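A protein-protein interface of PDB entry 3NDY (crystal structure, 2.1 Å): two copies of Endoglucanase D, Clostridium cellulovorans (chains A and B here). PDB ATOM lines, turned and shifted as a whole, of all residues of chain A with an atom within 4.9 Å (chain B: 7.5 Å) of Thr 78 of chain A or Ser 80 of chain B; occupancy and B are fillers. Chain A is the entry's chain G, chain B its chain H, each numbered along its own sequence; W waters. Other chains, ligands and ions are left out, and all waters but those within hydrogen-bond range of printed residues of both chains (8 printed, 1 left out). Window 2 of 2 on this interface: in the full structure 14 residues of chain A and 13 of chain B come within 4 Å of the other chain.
The side-chain amino group of Lys 24 of chain A sits at hydrogen-bond distance from the side-chain hydroxyl of Ser 51 of chain B (3.2 Å). The side-chain hydroxyl (OG1) of Thr 22 of chain A is in hydrogen-bond range of the side-chain hydroxyl (OG1) of Thr 22 of chain B, 3.4 Å away. The side-chain hydroxyl (OG) of Ser 80 of chain B lies within hydrogen-bond range of the side-chain hydroxyl (OG) of Ser 80 of chain A, at 3.4 Å. OG1 of Thr 22 of chain A is in hydrogen-bond range of OD1 of Asn 20 of chain B (3.1 Å).
Thr 22 of chain B touches its own counterpart, Thr 22 of chain A. Thr 22 of chain A touches Ser 80 of chain B, and with the chains exchanged Ser 80 of chain A touches Thr 22 of chain B. Thr 78 of chain A touches Ser 80 of chain B, but with the chains exchanged Ser 80 of chain A does not touch Thr 78 of chain B (4.2 Å). Ser 80 of chain B touches its own counterpart, Ser 80 of chain A. Positions printed for both chains: 22, 23, 72, 78, 79 and 80. Of the 7 pairs that touch across the chains among the printed residues, 4 have their exchanged pair printed and touching as well.
Printed residues of chain B within 4 Å of Lys 24 of chain A: Ser 51. Printed residues of chain B within 4 Å of Thr 78 of chain A: Ser 80 (3.99 Å). Gln 79 of chain A touches none of the printed residues of chain B. Of the printed residues of chain B, Ser 80 of chain A touches Thr 22 (3.6 Å) and Ser 80 (3.4 Å). Of the printed residues of chain A, Asn 20 of chain B touches Thr 22 (3.1 Å). Of the printed residues of chain A, Thr 22 of chain B touches Thr 22 (3.4 Å) and Ser 80 (3.6 Å). Of the printed residues of chain A, Ser 51 of chain B touches Lys 24. Printed residues of chain A within 4 Å of Ser 80 of chain B: Thr 22, Thr 78 and Ser 80. The nearest printed residue of chain B that does not touch Thr 78 of chain A is Gln 79 of chain B (4.2 Å). The nearest printed residue of chain A that does not touch Ser 80 of chain B is Lys 24 of chain A (5.3 Å).
Of the 10 printed residues of chain A, 4 touch a printed residue of chain B. Printed residues of chain A that touch a printed residue of chain B: Thr 22, Lys 24, Thr 78 and Ser 80. Among the printed residues, 7 pairs touch across the chains.
Water W6 lies within hydrogen-bond range of the side-chain amide oxygen (OE1) of Gln 79 of chain B, the side-chain hydroxyl (OG1) of Thr 78 of chain A and the backbone NH (N) of Ser 80 of chain B. Water W4 bridges the backbone carbonyl oxygen (O) of Thr 78 of chain A (2.7 Å) and the backbone carbonyl oxygen (O) of Thr 78 of chain B (2.8 Å). Water W1 lies within hydrogen-bond range of OE1 of Gln 79 of chain B (2.8 Å) and N of Thr 78 of chain A (3.0 Å). Water W8 lies within hydrogen-bond range of OG1 of Thr 78 of chain A, OG of Ser 80 of chain B, OG1 of Thr 78 of chain B and OG of Ser 80 of chain A. Water W2 bridges the side-chain amide oxygen of Gln 79 of chain A (2.9 Å) and the backbone NH of Thr 78 of chain B (2.9 Å). Water W7 lies within hydrogen-bond range of the side-chain amide oxygen of Asn 20 of chain B (3.0 Å) and the side-chain hydroxyl of Thr 22 of chain A (3.2 Å).
Among the printed residues, merely in contact across the chains: Thr 22 of chain A with Ser 80 of chain B (3.6 Å), Thr 78 of chain A with Ser 80 of chain B (3.99 Å) and Ser 80 of chain A with Thr 22 of chain B (3.6 Å).
The side-chain hydroxyl of Ser 80 of chain B sits at hydrogen-bond distance from the side-chain hydroxyl of Thr 22 of chain B (2.9 Å). N of Thr 6 of chain B sits at hydrogen-bond distance from O of Thr 22 of chain B, at 2.8 Å. The side-chain hydroxyl of Ser 80 of chain A sits at hydrogen-bond distance from the side-chain hydroxyl of Thr 22 of chain A (2.8 Å). O of Ser 51 of chain B is in hydrogen-bond range of ND2 of Asn 69 of chain B.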
ATOM      1  N   THR A  22     -20.619 -17.810   8.796  1.00  0.00           N
ATOM      2  CA  THR A  22     -19.221 -17.921   9.207  1.00  0.00           C
ATOM      3  C   THR A  22     -18.446 -18.801   8.224  1.00  0.00           C
ATOM      4  O   THR A  22     -18.832 -19.939   7.956  1.00  0.00           O
ATOM      5  CB  THR A  22     -19.084 -18.490  10.647  1.00  0.00           C
ATOM      6  OG1 THR A  22     -19.720 -17.605  11.583  1.00  0.00           O
ATOM      7  CG2 THR A  22     -17.613 -18.639  11.029  1.00  0.00           C
ATOM      8  N   ILE A  23     -17.364 -18.270   7.669  1.00  0.00           N
ATOM      9  CA  ILE A  23     -16.517 -19.052   6.766  1.00  0.00           C
ATOM     10  C   ILE A  23     -15.277 -19.453   7.534  1.00  0.00           C
ATOM     11  O   ILE A  23     -14.603 -18.601   8.129  1.00  0.00           O
ATOM     12  CB  ILE A  23     -16.093 -18.252   5.514  1.00  0.00           C
ATOM     13  CG1 ILE A  23     -17.302 -17.587   4.854  1.00  0.00           C
ATOM     14  CG2 ILE A  23     -15.320 -19.154   4.525  1.00  0.00           C
ATOM     15  CD1 ILE A  23     -16.926 -16.675   3.716  1.00  0.00           C
ATOM     16  N   LYS A  24     -14.985 -20.750   7.550  1.00  0.00           N
ATOM     17  CA  LYS A  24     -13.856 -21.246   8.326  1.00  0.00           C
ATOM     18  C   LYS A  24     -12.837 -21.933   7.421  1.00  0.00           C
ATOM     19  O   LYS A  24     -13.189 -22.844   6.660  1.00  0.00           O
ATOM     20  CB  LYS A  24     -14.342 -22.223   9.399  1.00  0.00           C
ATOM     21  CG  LYS A  24     -13.223 -22.734  10.280  1.00  0.00           C
ATOM     22  CD  LYS A  24     -13.627 -24.059  10.897  1.00  0.00           C
ATOM     23  CE  LYS A  24     -13.169 -24.156  12.322  1.00  0.00           C
ATOM     24  NZ  LYS A  24     -13.950 -23.206  13.148  1.00  0.00           N
ATOM     25  N   ILE A  72      -9.086 -14.779   5.300  1.00  0.00           N
ATOM     26  CA  ILE A  72      -9.412 -15.890   6.177  1.00  0.00           C
ATOM     27  C   ILE A  72      -8.138 -16.673   6.503  1.00  0.00           C
ATOM     28  O   ILE A  72      -7.562 -17.356   5.641  1.00  0.00           O
ATOM     29  CB  ILE A  72     -10.528 -16.809   5.607  1.00  0.00           C
ATOM     30  CG1 ILE A  72     -11.638 -15.966   4.966  1.00  0.00           C
ATOM     31  CG2 ILE A  72     -11.142 -17.605   6.716  1.00  0.00           C
ATOM     32  CD1 ILE A  72     -12.758 -16.798   4.357  1.00  0.00           C
ATOM     33  N   ALA A  73      -7.691 -16.546   7.751  1.00  0.00           N
ATOM     34  CA  ALA A  73      -6.443 -17.163   8.185  1.00  0.00           C
ATOM     35  C   ALA A  73      -6.503 -18.679   8.104  1.00  0.00           C
ATOM     36  O   ALA A  73      -7.570 -19.294   8.282  1.00  0.00           O
ATOM     37  CB  ALA A  73      -6.063 -16.703   9.603  1.00  0.00           C
ATOM     38  N   GLY A  76      -7.827 -22.896  10.762  1.00  0.00           N
ATOM     39  CA  GLY A  76      -8.973 -22.617  11.616  1.00  0.00           C
ATOM     40  C   GLY A  76      -9.431 -21.171  11.682  1.00  0.00           C
ATOM     41  O   GLY A  76     -10.302 -20.836  12.477  1.00  0.00           O
ATOM     42  N   GLY A  77      -8.856 -20.302  10.860  1.00  0.00           N
ATOM     43  CA  GLY A  77      -9.268 -18.908  10.861  1.00  0.00           C
ATOM     44  C   GLY A  77     -10.700 -18.763  10.380  1.00  0.00           C
ATOM     45  O   GLY A  77     -11.180 -19.570   9.578  1.00  0.00           O
ATOM     46  N   THR A  78     -11.394 -17.741  10.867  1.00  0.00           N
ATOM     47  CA  THR A  78     -12.740 -17.460  10.383  1.00  0.00           C
ATOM     48  C   THR A  78     -12.917 -15.999   9.993  1.00  0.00           C
ATOM     49  O   THR A  78     -12.135 -15.127  10.387  1.00  0.00           O
ATOM     50  CB  THR A  78     -13.834 -17.801  11.432  1.00  0.00           C
ATOM     51  OG1 THR A  78     -13.706 -16.937  12.568  1.00  0.00           O
ATOM     52  CG2 THR A  78     -13.758 -19.276  11.863  1.00  0.00           C
ATOM     53  N   GLN A  79     -13.936 -15.757   9.174  1.00  0.00           N
ATOM     54  CA  GLN A  79     -14.511 -14.430   8.991  1.00  0.00           C
ATOM     55  C   GLN A  79     -16.033 -14.616   8.865  1.00  0.00           C
ATOM     56  O   GLN A  79     -16.496 -15.644   8.354  1.00  0.00           O
ATOM     57  CB  GLN A  79     -13.932 -13.716   7.762  1.00  0.00           C
ATOM     58  CG  GLN A  79     -12.420 -13.417   7.810  1.00  0.00           C
ATOM     59  CD  GLN A  79     -12.051 -12.306   8.792  1.00  0.00           C
ATOM     60  OE1 GLN A  79     -12.903 -11.789   9.509  1.00  0.00           O
ATOM     61  NE2 GLN A  79     -10.771 -11.940   8.827  1.00  0.00           N
ATOM     62  N   SER A  80     -16.794 -13.629   9.337  1.00  0.00           N
ATOM     63  CA  SER A  80     -18.255 -13.715   9.373  1.00  0.00           C
ATOM     64  C   SER A  80     -18.928 -12.464   8.817  1.00  0.00           C
ATOM     65  O   SER A  80     -18.375 -11.366   8.873  1.00  0.00           O
ATOM     66  CB  SER A  80     -18.746 -13.946  10.813  1.00  0.00           C
ATOM     67  OG  SER A  80     -18.277 -15.182  11.328  1.00  0.00           O
ATOM     68  N   THR B   6     -23.525 -12.564  18.297  1.00  0.00           N
ATOM     69  CA  THR B   6     -24.532 -13.130  17.419  1.00  0.00           C
ATOM     70  C   THR B   6     -24.663 -14.607  17.758  1.00  0.00           C
ATOM     71  O   THR B   6     -23.725 -15.384  17.569  1.00  0.00           O
ATOM     72  CB  THR B   6     -24.145 -12.951  15.939  1.00  0.00           C
ATOM     73  OG1 THR B   6     -24.072 -11.551  15.625  1.00  0.00           O
ATOM     74  CG2 THR B   6     -25.173 -13.602  15.033  1.00  0.00           C
ATOM     75  N   ASN B  20     -24.173 -21.649  16.351  1.00  0.00           N
ATOM     76  CA  ASN B  20     -22.950 -20.936  15.984  1.00  0.00           C
ATOM     77  C   ASN B  20     -22.951 -19.570  16.659  1.00  0.00           C
ATOM     78  O   ASN B  20     -23.954 -18.864  16.623  1.00  0.00           O
ATOM     79  CB  ASN B  20     -22.831 -20.779  14.466  1.00  0.00           C
ATOM     80  CG  ASN B  20     -21.474 -20.246  14.045  1.00  0.00           C
ATOM     81  OD1 ASN B  20     -21.319 -19.055  13.783  1.00  0.00           O
ATOM     82  ND2 ASN B  20     -20.477 -21.128  13.994  1.00  0.00           N
ATOM     83  N   VAL B  21     -21.848 -19.220  17.309  1.00  0.00           N
ATOM     84  CA  VAL B  21     -21.747 -17.945  18.016  1.00  0.00           C
ATOM     85  C   VAL B  21     -20.622 -17.118  17.398  1.00  0.00           C
ATOM     86  O   VAL B  21     -19.524 -17.613  17.195  1.00  0.00           O
ATOM     87  CB  VAL B  21     -21.436 -18.148  19.523  1.00  0.00           C
ATOM     88  CG1 VAL B  21     -21.393 -16.810  20.249  1.00  0.00           C
ATOM     89  CG2 VAL B  21     -22.447 -19.086  20.168  1.00  0.00           C
ATOM     90  N   THR B  22     -20.906 -15.861  17.098  1.00  0.00           N
ATOM     91  CA  THR B  22     -19.891 -14.961  16.569  1.00  0.00           C
ATOM     92  C   THR B  22     -19.777 -13.771  17.505  1.00  0.00           C
ATOM     93  O   THR B  22     -20.776 -13.132  17.830  1.00  0.00           O
ATOM     94  CB  THR B  22     -20.257 -14.471  15.171  1.00  0.00           C
ATOM     95  OG1 THR B  22     -20.310 -15.589  14.275  1.00  0.00           O
ATOM     96  CG2 THR B  22     -19.219 -13.451  14.660  1.00  0.00           C
ATOM     97  N   ILE B  23     -18.562 -13.494  17.959  1.00  0.00           N
ATOM     98  CA  ILE B  23     -18.324 -12.348  18.827  1.00  0.00           C
ATOM     99  C   ILE B  23     -17.635 -11.243  18.028  1.00  0.00           C
ATOM    100  O   ILE B  23     -16.631 -11.494  17.358  1.00  0.00           O
ATOM    101  CB  ILE B  23     -17.420 -12.705  20.014  1.00  0.00           C
ATOM    102  CG1 ILE B  23     -17.952 -13.927  20.774  1.00  0.00           C
ATOM    103  CG2 ILE B  23     -17.308 -11.505  20.933  1.00  0.00           C
ATOM    104  CD1 ILE B  23     -16.947 -14.527  21.771  1.00  0.00           C
ATOM    105  N   TRP B  34     -10.098 -14.155  24.861  1.00  0.00           N
ATOM    106  CA  TRP B  34     -11.514 -13.915  25.152  1.00  0.00           C
ATOM    107  C   TRP B  34     -12.198 -15.029  25.950  1.00  0.00           C
ATOM    108  O   TRP B  34     -11.895 -16.216  25.786  1.00  0.00           O
ATOM    109  CB  TRP B  34     -12.308 -13.614  23.870  1.00  0.00           C
ATOM    110  CG  TRP B  34     -12.426 -14.773  22.882  1.00  0.00           C
ATOM    111  CD1 TRP B  34     -11.685 -14.970  21.754  1.00  0.00           C
ATOM    112  CD2 TRP B  34     -13.353 -15.862  22.942  1.00  0.00           C
ATOM    113  NE1 TRP B  34     -12.087 -16.116  21.111  1.00  0.00           N
ATOM    114  CE2 TRP B  34     -13.109 -16.683  21.823  1.00  0.00           C
ATOM    115  CE3 TRP B  34     -14.354 -16.234  23.847  1.00  0.00           C
ATOM    116  CZ2 TRP B  34     -13.831 -17.841  21.578  1.00  0.00           C
ATOM    117  CZ3 TRP B  34     -15.066 -17.383  23.604  1.00  0.00           C
ATOM    118  CH2 TRP B  34     -14.809 -18.172  22.476  1.00  0.00           C
ATOM    119  N   TRP B  50     -16.843 -26.977  19.679  1.00  0.00           N
ATOM    120  CA  TRP B  50     -15.616 -26.875  18.898  1.00  0.00           C
ATOM    121  C   TRP B  50     -15.117 -25.423  18.804  1.00  0.00           C
ATOM    122  O   TRP B  50     -15.908 -24.476  18.866  1.00  0.00           O
ATOM    123  CB  TRP B  50     -15.819 -27.477  17.493  1.00  0.00           C
ATOM    124  CG  TRP B  50     -17.048 -26.954  16.805  1.00  0.00           C
ATOM    125  CD1 TRP B  50     -17.142 -25.847  16.001  1.00  0.00           C
ATOM    126  CD2 TRP B  50     -18.367 -27.507  16.882  1.00  0.00           C
ATOM    127  NE1 TRP B  50     -18.445 -25.684  15.567  1.00  0.00           N
ATOM    128  CE2 TRP B  50     -19.214 -26.688  16.096  1.00  0.00           C
ATOM    129  CE3 TRP B  50     -18.916 -28.615  17.537  1.00  0.00           C
ATOM    130  CZ2 TRP B  50     -20.581 -26.951  15.948  1.00  0.00           C
ATOM    131  CZ3 TRP B  50     -20.278 -28.873  17.386  1.00  0.00           C
ATOM    132  CH2 TRP B  50     -21.089 -28.043  16.599  1.00  0.00           C
ATOM    133  N   SER B  51     -13.802 -25.267  18.649  1.00  0.00           N
ATOM    134  CA  SER B  51     -13.143 -23.954  18.576  1.00  0.00           C
ATOM    135  C   SER B  51     -13.214 -23.172  19.881  1.00  0.00           C
ATOM    136  O   SER B  51     -12.943 -21.962  19.916  1.00  0.00           O
ATOM    137  CB  SER B  51     -13.700 -23.120  17.428  1.00  0.00           C
ATOM    138  OG  SER B  51     -13.633 -23.859  16.227  1.00  0.00           O
ATOM    139  N   ALA B  52     -13.557 -23.885  20.947  1.00  0.00           N
ATOM    140  CA  ALA B  52     -13.689 -23.314  22.279  1.00  0.00           C
ATOM    141  C   ALA B  52     -13.921 -24.469  23.245  1.00  0.00           C
ATOM    142  O   ALA B  52     -14.199 -25.593  22.821  1.00  0.00           O
ATOM    143  CB  ALA B  52     -14.858 -22.340  22.326  1.00  0.00           C
ATOM    144  N   TYR B  68      -5.608 -20.419  19.436  1.00  0.00           N
ATOM    145  CA  TYR B  68      -5.365 -19.907  18.088  1.00  0.00           C
ATOM    146  C   TYR B  68      -6.380 -18.834  17.681  1.00  0.00           C
ATOM    147  O   TYR B  68      -6.102 -18.016  16.806  1.00  0.00           O
ATOM    148  CB  TYR B  68      -5.342 -21.045  17.061  1.00  0.00           C
ATOM    149  CG  TYR B  68      -6.611 -21.873  17.015  1.00  0.00           C
ATOM    150  CD1 TYR B  68      -7.722 -21.453  16.286  1.00  0.00           C
ATOM    151  CD2 TYR B  68      -6.694 -23.084  17.691  1.00  0.00           C
ATOM    152  CE1 TYR B  68      -8.893 -22.227  16.246  1.00  0.00           C
ATOM    153  CE2 TYR B  68      -7.847 -23.857  17.647  1.00  0.00           C
ATOM    154  CZ  TYR B  68      -8.938 -23.419  16.925  1.00  0.00           C
ATOM    155  OH  TYR B  68     -10.081 -24.183  16.896  1.00  0.00           O
ATOM    156  N   ASN B  69      -7.549 -18.828  18.318  1.00  0.00           N
ATOM    157  CA  ASN B  69      -8.555 -17.796  18.046  1.00  0.00           C
ATOM    158  C   ASN B  69      -8.789 -16.883  19.261  1.00  0.00           C
ATOM    159  O   ASN B  69      -9.882 -16.345  19.440  1.00  0.00           O
ATOM    160  CB  ASN B  69      -9.878 -18.440  17.606  1.00  0.00           C
ATOM    161  CG  ASN B  69     -10.446 -19.388  18.658  1.00  0.00           C
ATOM    162  OD1 ASN B  69      -9.910 -19.491  19.764  1.00  0.00           O
ATOM    163  ND2 ASN B  69     -11.531 -20.078  18.319  1.00  0.00           N
ATOM    164  N   ILE B  72      -9.643 -11.168  19.765  1.00  0.00           N
ATOM    165  CA  ILE B  72     -10.653 -10.555  18.912  1.00  0.00           C
ATOM    166  C   ILE B  72     -10.168  -9.154  18.574  1.00  0.00           C
ATOM    167  O   ILE B  72     -10.136  -8.277  19.433  1.00  0.00           O
ATOM    168  CB  ILE B  72     -12.060 -10.525  19.579  1.00  0.00           C
ATOM    169  CG1 ILE B  72     -12.341 -11.867  20.286  1.00  0.00           C
ATOM    170  CG2 ILE B  72     -13.134 -10.232  18.515  1.00  0.00           C
ATOM    171  CD1 ILE B  72     -13.641 -11.921  21.022  1.00  0.00           C
ATOM    172  N   THR B  78     -13.686 -10.298  14.511  1.00  0.00           N
ATOM    173  CA  THR B  78     -14.531 -11.340  15.090  1.00  0.00           C
ATOM    174  C   THR B  78     -13.770 -12.624  15.409  1.00  0.00           C
ATOM    175  O   THR B  78     -12.658 -12.866  14.913  1.00  0.00           O
ATOM    176  CB  THR B  78     -15.663 -11.737  14.134  1.00  0.00           C
ATOM    177  OG1 THR B  78     -15.084 -12.301  12.952  1.00  0.00           O
ATOM    178  CG2 THR B  78     -16.519 -10.525  13.786  1.00  0.00           C
ATOM    179  N   GLN B  79     -14.383 -13.438  16.259  1.00  0.00           N
ATOM    180  CA  GLN B  79     -14.019 -14.840  16.410  1.00  0.00           C
ATOM    181  C   GLN B  79     -15.325 -15.601  16.609  1.00  0.00           C
ATOM    182  O   GLN B  79     -16.296 -15.040  17.104  1.00  0.00           O
ATOM    183  CB  GLN B  79     -13.069 -15.056  17.593  1.00  0.00           C
ATOM    184  CG  GLN B  79     -11.710 -14.345  17.476  1.00  0.00           C
ATOM    185  CD  GLN B  79     -10.794 -14.958  16.422  1.00  0.00           C
ATOM    186  OE1 GLN B  79     -11.165 -15.905  15.732  1.00  0.00           O
ATOM    187  NE2 GLN B  79      -9.587 -14.418  16.303  1.00  0.00           N
ATOM    188  N   SER B  80     -15.357 -16.864  16.195  1.00  0.00           N
ATOM    189  CA  SER B  80     -16.576 -17.665  16.261  1.00  0.00           C
ATOM    190  C   SER B  80     -16.287 -19.044  16.825  1.00  0.00           C
ATOM    191  O   SER B  80     -15.153 -19.524  16.764  1.00  0.00           O
ATOM    192  CB  SER B  80     -17.178 -17.842  14.863  1.00  0.00           C
ATOM    193  OG  SER B  80     -17.600 -16.602  14.347  1.00  0.00           O
ATOM    194  N   PHE B  81     -17.324 -19.682  17.359  1.00  0.00           N
ATOM    195  CA  PHE B  81     -17.232 -21.073  17.785  1.00  0.00           C
ATOM    196  C   PHE B  81     -18.623 -21.668  17.674  1.00  0.00           C
ATOM    197  O   PHE B  81     -19.581 -20.959  17.375  1.00  0.00           O
ATOM    198  CB  PHE B  81     -16.702 -21.180  19.220  1.00  0.00           C
ATOM    199  CG  PHE B  81     -17.638 -20.615  20.251  1.00  0.00           C
ATOM    200  CD1 PHE B  81     -18.508 -21.445  20.950  1.00  0.00           C
ATOM    201  CD2 PHE B  81     -17.658 -19.251  20.517  1.00  0.00           C
ATOM    202  CE1 PHE B  81     -19.381 -20.920  21.910  1.00  0.00           C
ATOM    203  CE2 PHE B  81     -18.525 -18.715  21.464  1.00  0.00           C
ATOM    204  CZ  PHE B  81     -19.388 -19.558  22.162  1.00  0.00           C
ATOM    205  N   GLY B  82     -18.747 -22.972  17.890  1.00  0.00           N
ATOM    206  CA  GLY B  82     -20.055 -23.596  17.793  1.00  0.00           C
ATOM    207  C   GLY B  82     -20.198 -24.764  18.734  1.00  0.00           C
ATOM    208  O   GLY B  82     -19.220 -25.243  19.295  1.00  0.00           O
HETATM  209  O   HOH W   1     -10.098 -16.456  13.240  1.00  0.00           O
HETATM  210  O   HOH W   2     -12.248 -10.531  11.992  1.00  0.00           O
HETATM  211  O   HOH W   3     -11.625 -22.297  14.060  1.00  0.00           O
HETATM  212  O   HOH W   4     -11.498 -13.441  12.428  1.00  0.00           O
HETATM  213  O   HOH W   5     -15.252 -11.437  10.459  1.00  0.00           O
HETATM  214  O   HOH W   6     -12.842 -17.805  14.947  1.00  0.00           O
HETATM  215  O   HOH W   7     -22.806 -18.290  11.331  1.00  0.00           O
HETATM  216  O   HOH W   8     -15.759 -15.085  12.768  1.00  0.00           O
